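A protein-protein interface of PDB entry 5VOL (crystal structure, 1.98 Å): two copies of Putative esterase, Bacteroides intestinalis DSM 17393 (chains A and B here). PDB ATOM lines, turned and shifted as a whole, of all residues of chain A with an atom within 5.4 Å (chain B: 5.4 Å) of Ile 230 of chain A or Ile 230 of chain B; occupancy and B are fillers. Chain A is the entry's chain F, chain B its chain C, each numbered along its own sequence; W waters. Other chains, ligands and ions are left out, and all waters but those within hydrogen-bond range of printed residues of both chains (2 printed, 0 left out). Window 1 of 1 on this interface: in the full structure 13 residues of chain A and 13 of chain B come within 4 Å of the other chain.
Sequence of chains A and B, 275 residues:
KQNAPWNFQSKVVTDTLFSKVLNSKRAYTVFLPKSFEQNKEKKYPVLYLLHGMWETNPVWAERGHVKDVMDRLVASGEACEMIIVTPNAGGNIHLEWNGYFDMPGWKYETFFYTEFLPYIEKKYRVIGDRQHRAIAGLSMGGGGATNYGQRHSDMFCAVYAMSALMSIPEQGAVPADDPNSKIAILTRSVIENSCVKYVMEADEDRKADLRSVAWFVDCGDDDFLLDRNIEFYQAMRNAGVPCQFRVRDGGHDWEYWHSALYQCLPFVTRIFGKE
Leu 226 of chain A touches Tyr 233 of chain B, and with the chains exchanged Tyr 233 of chain A touches Leu 226 of chain B.
Asp 227 of chain A touches Gln 234 of chain B, and with the chains exchanged Gln 234 of chain A touches Asp 227 of chain B.
Ile 230 of chain A touches its own counterpart, Ile 230 of chain B.
Ile 230 of chain A touches Gln 234 of chain B, and with the chains exchanged Gln 234 of chain A touches Ile 230 of chain B.
12 positions are printed for both chains.
Of the 7 pairs that touch across the chains among the printed residues, 7 have their exchanged pair printed and touching as well.
Water W1 bridges the backbone carbonyl oxygen (O) of Asp 227 of chain B (3.0 Å) and the side-chain amide nitrogen (NE2) of Gln 234 of chain A (3.1 Å).
Water W2 lies within hydrogen-bond range of the backbone carbonyl oxygen of Asp 227 of chain A, the side-chain amide nitrogen of Gln 234 of chain B and the side-chain carboxylate of Glu 231 of chain A.
Among the printed residues, merely in contact across the chains: Ile 230 of chain A with Ile 230 of chain B, Tyr 233 of chain A with Leu 226 of chain B, Leu 226 of chain A with Tyr 233 of chain B, Gln 234 of chain A with Ile 230 of chain B and Ile 230 of chain A with Gln 234 of chain B.
Of the printed residues of chain B, Ile 230 of chain A touches Ile 230 and Gln 234.
Of the printed residues of chain B, Leu 226 of chain A touches Tyr 233.
Printed residues of chain A within 4 Å of Leu 226 of chain B: Tyr 233 (3.8 Å).
Of the printed residues of chain B, Tyr 233 of chain A touches Leu 226 (3.8 Å).
The nearest printed residue of chain A that does not touch Asp 227 of chain B is Ile 230 of chain A (6.0 Å).
Of the 12 printed residues of chain A, 5 touch a printed residue of chain B.
Printed residues of chain B that touch a printed residue of chain A: Leu 226, Asp 227, Ile 230, Tyr 233 and Gln 234.
Among the printed residues, 7 pairs touch across the chains.
The side-chain amide nitrogen of Gln 234 of chain A lies within hydrogen-bond range of the side-chain carboxylate of Asp 227 of chain B (2.7 Å).
NE2 of Gln 234 of chain B sits at hydrogen-bond distance from OD1 of Asp 227 of chain A (2.7 Å).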
ATOM      1  N   LEU A 225      -5.736   6.482   5.186  1.00  0.00           N
ATOM      2  CA  LEU A 225      -5.206   7.799   4.840  1.00  0.00           C
ATOM      3  C   LEU A 225      -6.291   8.883   4.714  1.00  0.00           C
ATOM      4  O   LEU A 225      -5.997  10.018   4.346  1.00  0.00           O
ATOM      5  CB  LEU A 225      -4.408   7.719   3.534  1.00  0.00           C
ATOM      6  CG  LEU A 225      -3.024   7.081   3.654  1.00  0.00           C
ATOM      7  CD1 LEU A 225      -2.410   6.836   2.276  1.00  0.00           C
ATOM      8  CD2 LEU A 225      -2.144   8.026   4.461  1.00  0.00           C
ATOM      9  N   LEU A 226      -7.535   8.527   5.003  1.00  0.00           N
ATOM     10  CA  LEU A 226      -8.632   9.478   4.928  1.00  0.00           C
ATOM     11  C   LEU A 226      -8.361  10.721   5.779  1.00  0.00           C
ATOM     12  O   LEU A 226      -8.599  11.830   5.327  1.00  0.00           O
ATOM     13  CB  LEU A 226      -9.947   8.835   5.376  1.00  0.00           C
ATOM     14  CG  LEU A 226     -11.153   9.794   5.398  1.00  0.00           C
ATOM     15  CD1 LEU A 226     -11.476  10.314   3.995  1.00  0.00           C
ATOM     16  CD2 LEU A 226     -12.359   9.115   6.005  1.00  0.00           C
ATOM     17  N   ASP A 227      -7.865  10.539   7.002  1.00  0.00           N
ATOM     18  CA  ASP A 227      -7.680  11.692   7.883  1.00  0.00           C
ATOM     19  C   ASP A 227      -6.641  12.672   7.338  1.00  0.00           C
ATOM     20  O   ASP A 227      -6.839  13.876   7.450  1.00  0.00           O
ATOM     21  CB  ASP A 227      -7.305  11.257   9.306  1.00  0.00           C
ATOM     22  CG  ASP A 227      -8.469  10.617  10.054  1.00  0.00           C
ATOM     23  OD1 ASP A 227      -9.619  10.702   9.579  1.00  0.00           O
ATOM     24  OD2 ASP A 227      -8.239  10.029  11.132  1.00  0.00           O
ATOM     25  N   ARG A 228      -5.561  12.185   6.716  1.00  0.00           N
ATOM     26  CA  ARG A 228      -4.575  13.097   6.134  1.00  0.00           C
ATOM     27  C   ARG A 228      -5.113  13.834   4.903  1.00  0.00           C
ATOM     28  O   ARG A 228      -4.790  15.002   4.661  1.00  0.00           O
ATOM     29  CB  ARG A 228      -3.296  12.352   5.758  1.00  0.00           C
ATOM     30  CG  ARG A 228      -2.490  11.893   6.950  1.00  0.00           C
ATOM     31  CD  ARG A 228      -2.019  13.089   7.768  1.00  0.00           C
ATOM     32  NE  ARG A 228      -1.324  12.654   8.969  1.00  0.00           N
ATOM     33  CZ  ARG A 228      -0.772  13.471   9.858  1.00  0.00           C
ATOM     34  NH1 ARG A 228      -0.829  14.787   9.685  1.00  0.00           N
ATOM     35  NH2 ARG A 228      -0.165  12.966  10.924  1.00  0.00           N
ATOM     36  N   ASN A 229      -5.931  13.150   4.117  1.00  0.00           N
ATOM     37  CA  ASN A 229      -6.564  13.797   2.979  1.00  0.00           C
ATOM     38  C   ASN A 229      -7.586  14.852   3.394  1.00  0.00           C
ATOM     39  O   ASN A 229      -7.704  15.891   2.745  1.00  0.00           O
ATOM     40  CB  ASN A 229      -7.212  12.756   2.091  1.00  0.00           C
ATOM     41  CG  ASN A 229      -6.202  12.067   1.228  1.00  0.00           C
ATOM     42  OD1 ASN A 229      -5.803  12.609   0.203  1.00  0.00           O
ATOM     43  ND2 ASN A 229      -5.729  10.895   1.665  1.00  0.00           N
ATOM     44  N   ILE A 230      -8.316  14.571   4.466  1.00  0.00           N
ATOM     45  CA  ILE A 230      -9.227  15.556   5.050  1.00  0.00           C
ATOM     46  C   ILE A 230      -8.456  16.810   5.486  1.00  0.00           C
ATOM     47  O   ILE A 230      -8.884  17.947   5.225  1.00  0.00           O
ATOM     48  CB  ILE A 230      -9.999  14.962   6.253  1.00  0.00           C
ATOM     49  CG1 ILE A 230     -11.040  13.953   5.754  1.00  0.00           C
ATOM     50  CG2 ILE A 230     -10.673  16.078   7.074  1.00  0.00           C
ATOM     51  CD1 ILE A 230     -11.702  13.109   6.864  1.00  0.00           C
ATOM     52  N   GLU A 231      -7.316  16.603   6.140  1.00  0.00           N
ATOM     53  CA  GLU A 231      -6.489  17.729   6.578  1.00  0.00           C
ATOM     54  C   GLU A 231      -6.035  18.550   5.393  1.00  0.00           C
ATOM     55  O   GLU A 231      -6.007  19.782   5.460  1.00  0.00           O
ATOM     56  CB  GLU A 231      -5.279  17.244   7.377  1.00  0.00           C
ATOM     57  CG  GLU A 231      -5.632  16.828   8.777  1.00  0.00           C
ATOM     58  CD  GLU A 231      -4.556  15.979   9.435  1.00  0.00           C
ATOM     59  OE1 GLU A 231      -3.358  16.191   9.150  1.00  0.00           O
ATOM     60  OE2 GLU A 231      -4.919  15.092  10.238  1.00  0.00           O
ATOM     61  N   PHE A 232      -5.691  17.867   4.305  1.00  0.00           N
ATOM     62  CA  PHE A 232      -5.235  18.527   3.093  1.00  0.00           C
ATOM     63  C   PHE A 232      -6.354  19.350   2.473  1.00  0.00           C
ATOM     64  O   PHE A 232      -6.149  20.495   2.064  1.00  0.00           O
ATOM     65  CB  PHE A 232      -4.714  17.502   2.075  1.00  0.00           C
ATOM     66  CG  PHE A 232      -4.363  18.097   0.742  1.00  0.00           C
ATOM     67  CD1 PHE A 232      -3.084  18.568   0.492  1.00  0.00           C
ATOM     68  CD2 PHE A 232      -5.313  18.189  -0.270  1.00  0.00           C
ATOM     69  CE1 PHE A 232      -2.760  19.126  -0.743  1.00  0.00           C
ATOM     70  CE2 PHE A 232      -4.995  18.739  -1.501  1.00  0.00           C
ATOM     71  CZ  PHE A 232      -3.717  19.207  -1.743  1.00  0.00           C
ATOM     72  N   TYR A 233      -7.538  18.764   2.387  1.00  0.00           N
ATOM     73  CA  TYR A 233      -8.656  19.469   1.791  1.00  0.00           C
ATOM     74  C   TYR A 233      -9.047  20.678   2.636  1.00  0.00           C
ATOM     75  O   TYR A 233      -9.325  21.744   2.100  1.00  0.00           O
ATOM     76  CB  TYR A 233      -9.859  18.552   1.617  1.00  0.00           C
ATOM     77  CG  TYR A 233     -11.044  19.301   1.087  1.00  0.00           C
ATOM     78  CD1 TYR A 233     -10.982  19.943  -0.150  1.00  0.00           C
ATOM     79  CD2 TYR A 233     -12.212  19.399   1.823  1.00  0.00           C
ATOM     80  CE1 TYR A 233     -12.065  20.653  -0.644  1.00  0.00           C
ATOM     81  CE2 TYR A 233     -13.301  20.120   1.339  1.00  0.00           C
ATOM     82  CZ  TYR A 233     -13.220  20.735   0.106  1.00  0.00           C
ATOM     83  OH  TYR A 233     -14.297  21.448  -0.378  1.00  0.00           O
ATOM     84  N   GLN A 234      -9.066  20.497   3.953  1.00  0.00           N
ATOM     85  CA  GLN A 234      -9.434  21.570   4.872  1.00  0.00           C
ATOM     86  C   GLN A 234      -8.446  22.733   4.767  1.00  0.00           C
ATOM     87  O   GLN A 234      -8.844  23.898   4.750  1.00  0.00           O
ATOM     88  CB  GLN A 234      -9.515  21.039   6.304  1.00  0.00           C
ATOM     89  CG  GLN A 234     -10.775  20.214   6.541  1.00  0.00           C
ATOM     90  CD  GLN A 234     -10.857  19.590   7.918  1.00  0.00           C
ATOM     91  OE1 GLN A 234      -9.845  19.285   8.544  1.00  0.00           O
ATOM     92  NE2 GLN A 234     -12.078  19.403   8.401  1.00  0.00           N
ATOM     93  N   ALA A 235      -7.163  22.417   4.659  1.00  0.00           N
ATOM     94  CA  ALA A 235      -6.142  23.443   4.464  1.00  0.00           C
ATOM     95  C   ALA A 235      -6.350  24.195   3.154  1.00  0.00           C
ATOM     96  O   ALA A 235      -6.261  25.423   3.114  1.00  0.00           O
ATOM     97  CB  ALA A 235      -4.751  22.825   4.505  1.00  0.00           C
ATOM     98  N   PHE A 245     -13.378  17.568  -3.556  1.00  0.00           N
ATOM     99  CA  PHE A 245     -13.133  16.533  -2.567  1.00  0.00           C
ATOM    100  C   PHE A 245     -14.236  15.496  -2.684  1.00  0.00           C
ATOM    101  O   PHE A 245     -15.426  15.835  -2.661  1.00  0.00           O
ATOM    102  CB  PHE A 245     -13.082  17.141  -1.146  1.00  0.00           C
ATOM    103  CG  PHE A 245     -12.647  16.179  -0.062  1.00  0.00           C
ATOM    104  CD1 PHE A 245     -11.653  15.242  -0.291  1.00  0.00           C
ATOM    105  CD2 PHE A 245     -13.221  16.238   1.193  1.00  0.00           C
ATOM    106  CE1 PHE A 245     -11.257  14.370   0.714  1.00  0.00           C
ATOM    107  CE2 PHE A 245     -12.826  15.382   2.206  1.00  0.00           C
ATOM    108  CZ  PHE A 245     -11.841  14.442   1.967  1.00  0.00           C
ATOM    109  N   LEU B 225     -21.237  22.648   6.986  1.00  0.00           N
ATOM    110  CA  LEU B 225     -21.307  21.660   8.058  1.00  0.00           C
ATOM    111  C   LEU B 225     -20.422  20.426   7.815  1.00  0.00           C
ATOM    112  O   LEU B 225     -20.480  19.468   8.588  1.00  0.00           O
ATOM    113  CB  LEU B 225     -22.762  21.220   8.285  1.00  0.00           C
ATOM    114  CG  LEU B 225     -23.626  22.223   9.055  1.00  0.00           C
ATOM    115  CD1 LEU B 225     -25.103  21.838   9.049  1.00  0.00           C
ATOM    116  CD2 LEU B 225     -23.120  22.322  10.489  1.00  0.00           C
ATOM    117  N   LEU B 226     -19.598  20.451   6.771  1.00  0.00           N
ATOM    118  CA  LEU B 226     -18.726  19.314   6.468  1.00  0.00           C
ATOM    119  C   LEU B 226     -17.796  18.995   7.641  1.00  0.00           C
ATOM    120  O   LEU B 226     -17.644  17.840   8.025  1.00  0.00           O
ATOM    121  CB  LEU B 226     -17.899  19.568   5.198  1.00  0.00           C
ATOM    122  CG  LEU B 226     -16.892  18.450   4.853  1.00  0.00           C
ATOM    123  CD1 LEU B 226     -17.575  17.114   4.584  1.00  0.00           C
ATOM    124  CD2 LEU B 226     -16.024  18.818   3.658  1.00  0.00           C
ATOM    125  N   ASP B 227     -17.189  20.021   8.228  1.00  0.00           N
ATOM    126  CA  ASP B 227     -16.196  19.785   9.269  1.00  0.00           C
ATOM    127  C   ASP B 227     -16.781  19.073  10.494  1.00  0.00           C
ATOM    128  O   ASP B 227     -16.127  18.192  11.071  1.00  0.00           O
ATOM    129  CB  ASP B 227     -15.529  21.109   9.669  1.00  0.00           C
ATOM    130  CG  ASP B 227     -14.467  21.549   8.668  1.00  0.00           C
ATOM    131  OD1 ASP B 227     -14.256  20.836   7.656  1.00  0.00           O
ATOM    132  OD2 ASP B 227     -13.840  22.611   8.882  1.00  0.00           O
ATOM    133  N   ARG B 228     -18.004  19.422  10.888  1.00  0.00           N
ATOM    134  CA  ARG B 228     -18.639  18.747  12.021  1.00  0.00           C
ATOM    135  C   ARG B 228     -19.053  17.312  11.687  1.00  0.00           C
ATOM    136  O   ARG B 228     -19.067  16.444  12.560  1.00  0.00           O
ATOM    137  CB  ARG B 228     -19.869  19.514  12.503  1.00  0.00           C
ATOM    138  CG  ARG B 228     -19.561  20.865  13.122  1.00  0.00           C
ATOM    139  CD  ARG B 228     -18.546  20.759  14.236  1.00  0.00           C
ATOM    140  NE  ARG B 228     -18.498  21.988  15.039  1.00  0.00           N
ATOM    141  CZ  ARG B 228     -17.414  22.426  15.670  1.00  0.00           C
ATOM    142  NH1 ARG B 228     -16.274  21.743  15.601  1.00  0.00           N
ATOM    143  NH2 ARG B 228     -17.465  23.556  16.369  1.00  0.00           N
ATOM    144  N   ASN B 229     -19.444  17.074  10.439  1.00  0.00           N
ATOM    145  CA  ASN B 229     -19.838  15.718  10.042  1.00  0.00           C
ATOM    146  C   ASN B 229     -18.608  14.827  10.002  1.00  0.00           C
ATOM    147  O   ASN B 229     -18.673  13.639  10.318  1.00  0.00           O
ATOM    148  CB  ASN B 229     -20.565  15.728   8.695  1.00  0.00           C
ATOM    149  CG  ASN B 229     -22.025  16.046   8.841  1.00  0.00           C
ATOM    150  OD1 ASN B 229     -22.820  15.185   9.220  1.00  0.00           O
ATOM    151  ND2 ASN B 229     -22.388  17.307   8.600  1.00  0.00           N
ATOM    152  N   ILE B 230     -17.481  15.420   9.634  1.00  0.00           N
ATOM    153  CA  ILE B 230     -16.215  14.718   9.647  1.00  0.00           C
ATOM    154  C   ILE B 230     -15.861  14.314  11.073  1.00  0.00           C
ATOM    155  O   ILE B 230     -15.451  13.173  11.321  1.00  0.00           O
ATOM    156  CB  ILE B 230     -15.087  15.579   9.031  1.00  0.00           C
ATOM    157  CG1 ILE B 230     -15.229  15.614   7.501  1.00  0.00           C
ATOM    158  CG2 ILE B 230     -13.729  15.049   9.453  1.00  0.00           C
ATOM    159  CD1 ILE B 230     -14.263  16.578   6.789  1.00  0.00           C
ATOM    160  N   GLU B 231     -16.024  15.240  12.018  1.00  0.00           N
ATOM    161  CA  GLU B 231     -15.727  14.932  13.412  1.00  0.00           C
ATOM    162  C   GLU B 231     -16.626  13.820  13.924  1.00  0.00           C
ATOM    163  O   GLU B 231     -16.193  12.956  14.688  1.00  0.00           O
ATOM    164  CB  GLU B 231     -15.898  16.173  14.309  1.00  0.00           C
ATOM    165  CG  GLU B 231     -14.948  17.305  14.024  1.00  0.00           C
ATOM    166  CD  GLU B 231     -15.309  18.547  14.840  1.00  0.00           C
ATOM    167  OE1 GLU B 231     -15.788  18.394  15.987  1.00  0.00           O
ATOM    168  OE2 GLU B 231     -15.142  19.664  14.326  1.00  0.00           O
ATOM    169  N   PHE B 232     -17.893  13.855  13.537  1.00  0.00           N
ATOM    170  CA  PHE B 232     -18.798  12.794  13.937  1.00  0.00           C
ATOM    171  C   PHE B 232     -18.322  11.451  13.378  1.00  0.00           C
ATOM    172  O   PHE B 232     -18.257  10.448  14.096  1.00  0.00           O
ATOM    173  CB  PHE B 232     -20.215  13.086  13.456  1.00  0.00           C
ATOM    174  CG  PHE B 232     -21.174  11.961  13.696  1.00  0.00           C
ATOM    175  CD1 PHE B 232     -21.848  11.851  14.900  1.00  0.00           C
ATOM    176  CD2 PHE B 232     -21.395  11.001  12.718  1.00  0.00           C
ATOM    177  CE1 PHE B 232     -22.734  10.810  15.123  1.00  0.00           C
ATOM    178  CE2 PHE B 232     -22.281   9.964  12.933  1.00  0.00           C
ATOM    179  CZ  PHE B 232     -22.949   9.865  14.133  1.00  0.00           C
ATOM    180  N   TYR B 233     -17.989  11.429  12.093  1.00  0.00           N
ATOM    181  CA  TYR B 233     -17.560  10.176  11.480  1.00  0.00           C
ATOM    182  C   TYR B 233     -16.274   9.667  12.136  1.00  0.00           C
ATOM    183  O   TYR B 233     -16.181   8.498  12.509  1.00  0.00           O
ATOM    184  CB  TYR B 233     -17.353  10.324   9.964  1.00  0.00           C
ATOM    185  CG  TYR B 233     -16.867   9.022   9.362  1.00  0.00           C
ATOM    186  CD1 TYR B 233     -17.631   7.859   9.478  1.00  0.00           C
ATOM    187  CD2 TYR B 233     -15.636   8.940   8.727  1.00  0.00           C
ATOM    188  CE1 TYR B 233     -17.187   6.655   8.960  1.00  0.00           C
ATOM    189  CE2 TYR B 233     -15.183   7.740   8.201  1.00  0.00           C
ATOM    190  CZ  TYR B 233     -15.961   6.606   8.326  1.00  0.00           C
ATOM    191  OH  TYR B 233     -15.508   5.414   7.809  1.00  0.00           O
ATOM    192  N   GLN B 234     -15.285  10.544  12.281  1.00  0.00           N
ATOM    193  CA  GLN B 234     -14.031  10.168  12.926  1.00  0.00           C
ATOM    194  C   GLN B 234     -14.272   9.597  14.332  1.00  0.00           C
ATOM    195  O   GLN B 234     -13.705   8.556  14.681  1.00  0.00           O
ATOM    196  CB  GLN B 234     -13.074  11.361  12.966  1.00  0.00           C
ATOM    197  CG  GLN B 234     -12.493  11.687  11.579  1.00  0.00           C
ATOM    198  CD  GLN B 234     -11.668  12.956  11.548  1.00  0.00           C
ATOM    199  OE1 GLN B 234     -11.963  13.930  12.255  1.00  0.00           O
ATOM    200  NE2 GLN B 234     -10.627  12.964  10.709  1.00  0.00           N
ATOM    201  N   ALA B 235     -15.140  10.236  15.115  1.00  0.00           N
ATOM    202  CA  ALA B 235     -15.479   9.711  16.447  1.00  0.00           C
ATOM    203  C   ALA B 235     -16.122   8.321  16.369  1.00  0.00           C
ATOM    204  O   ALA B 235     -15.781   7.429  17.141  1.00  0.00           O
ATOM    205  CB  ALA B 235     -16.400  10.673  17.189  1.00  0.00           C
ATOM    206  N   PHE B 245     -19.771   6.786   5.336  1.00  0.00           N
ATOM    207  CA  PHE B 245     -19.548   8.226   5.178  1.00  0.00           C
ATOM    208  C   PHE B 245     -19.378   8.519   3.687  1.00  0.00           C
ATOM    209  O   PHE B 245     -18.581   7.866   3.022  1.00  0.00           O
ATOM    210  CB  PHE B 245     -18.315   8.664   5.980  1.00  0.00           C
ATOM    211  CG  PHE B 245     -18.078  10.168   6.009  1.00  0.00           C
ATOM    212  CD1 PHE B 245     -19.127  11.053   6.189  1.00  0.00           C
ATOM    213  CD2 PHE B 245     -16.795  10.682   5.865  1.00  0.00           C
ATOM    214  CE1 PHE B 245     -18.906  12.439   6.214  1.00  0.00           C
ATOM    215  CE2 PHE B 245     -16.559  12.067   5.903  1.00  0.00           C
ATOM    216  CZ  PHE B 245     -17.614  12.944   6.073  1.00  0.00           C
HETATM  217  O   HOH W   1     -13.173  18.259  11.099  1.00  0.00           O
HETATM  218  O   HOH W   2      -8.368  14.877   9.796  1.00  0.00           O
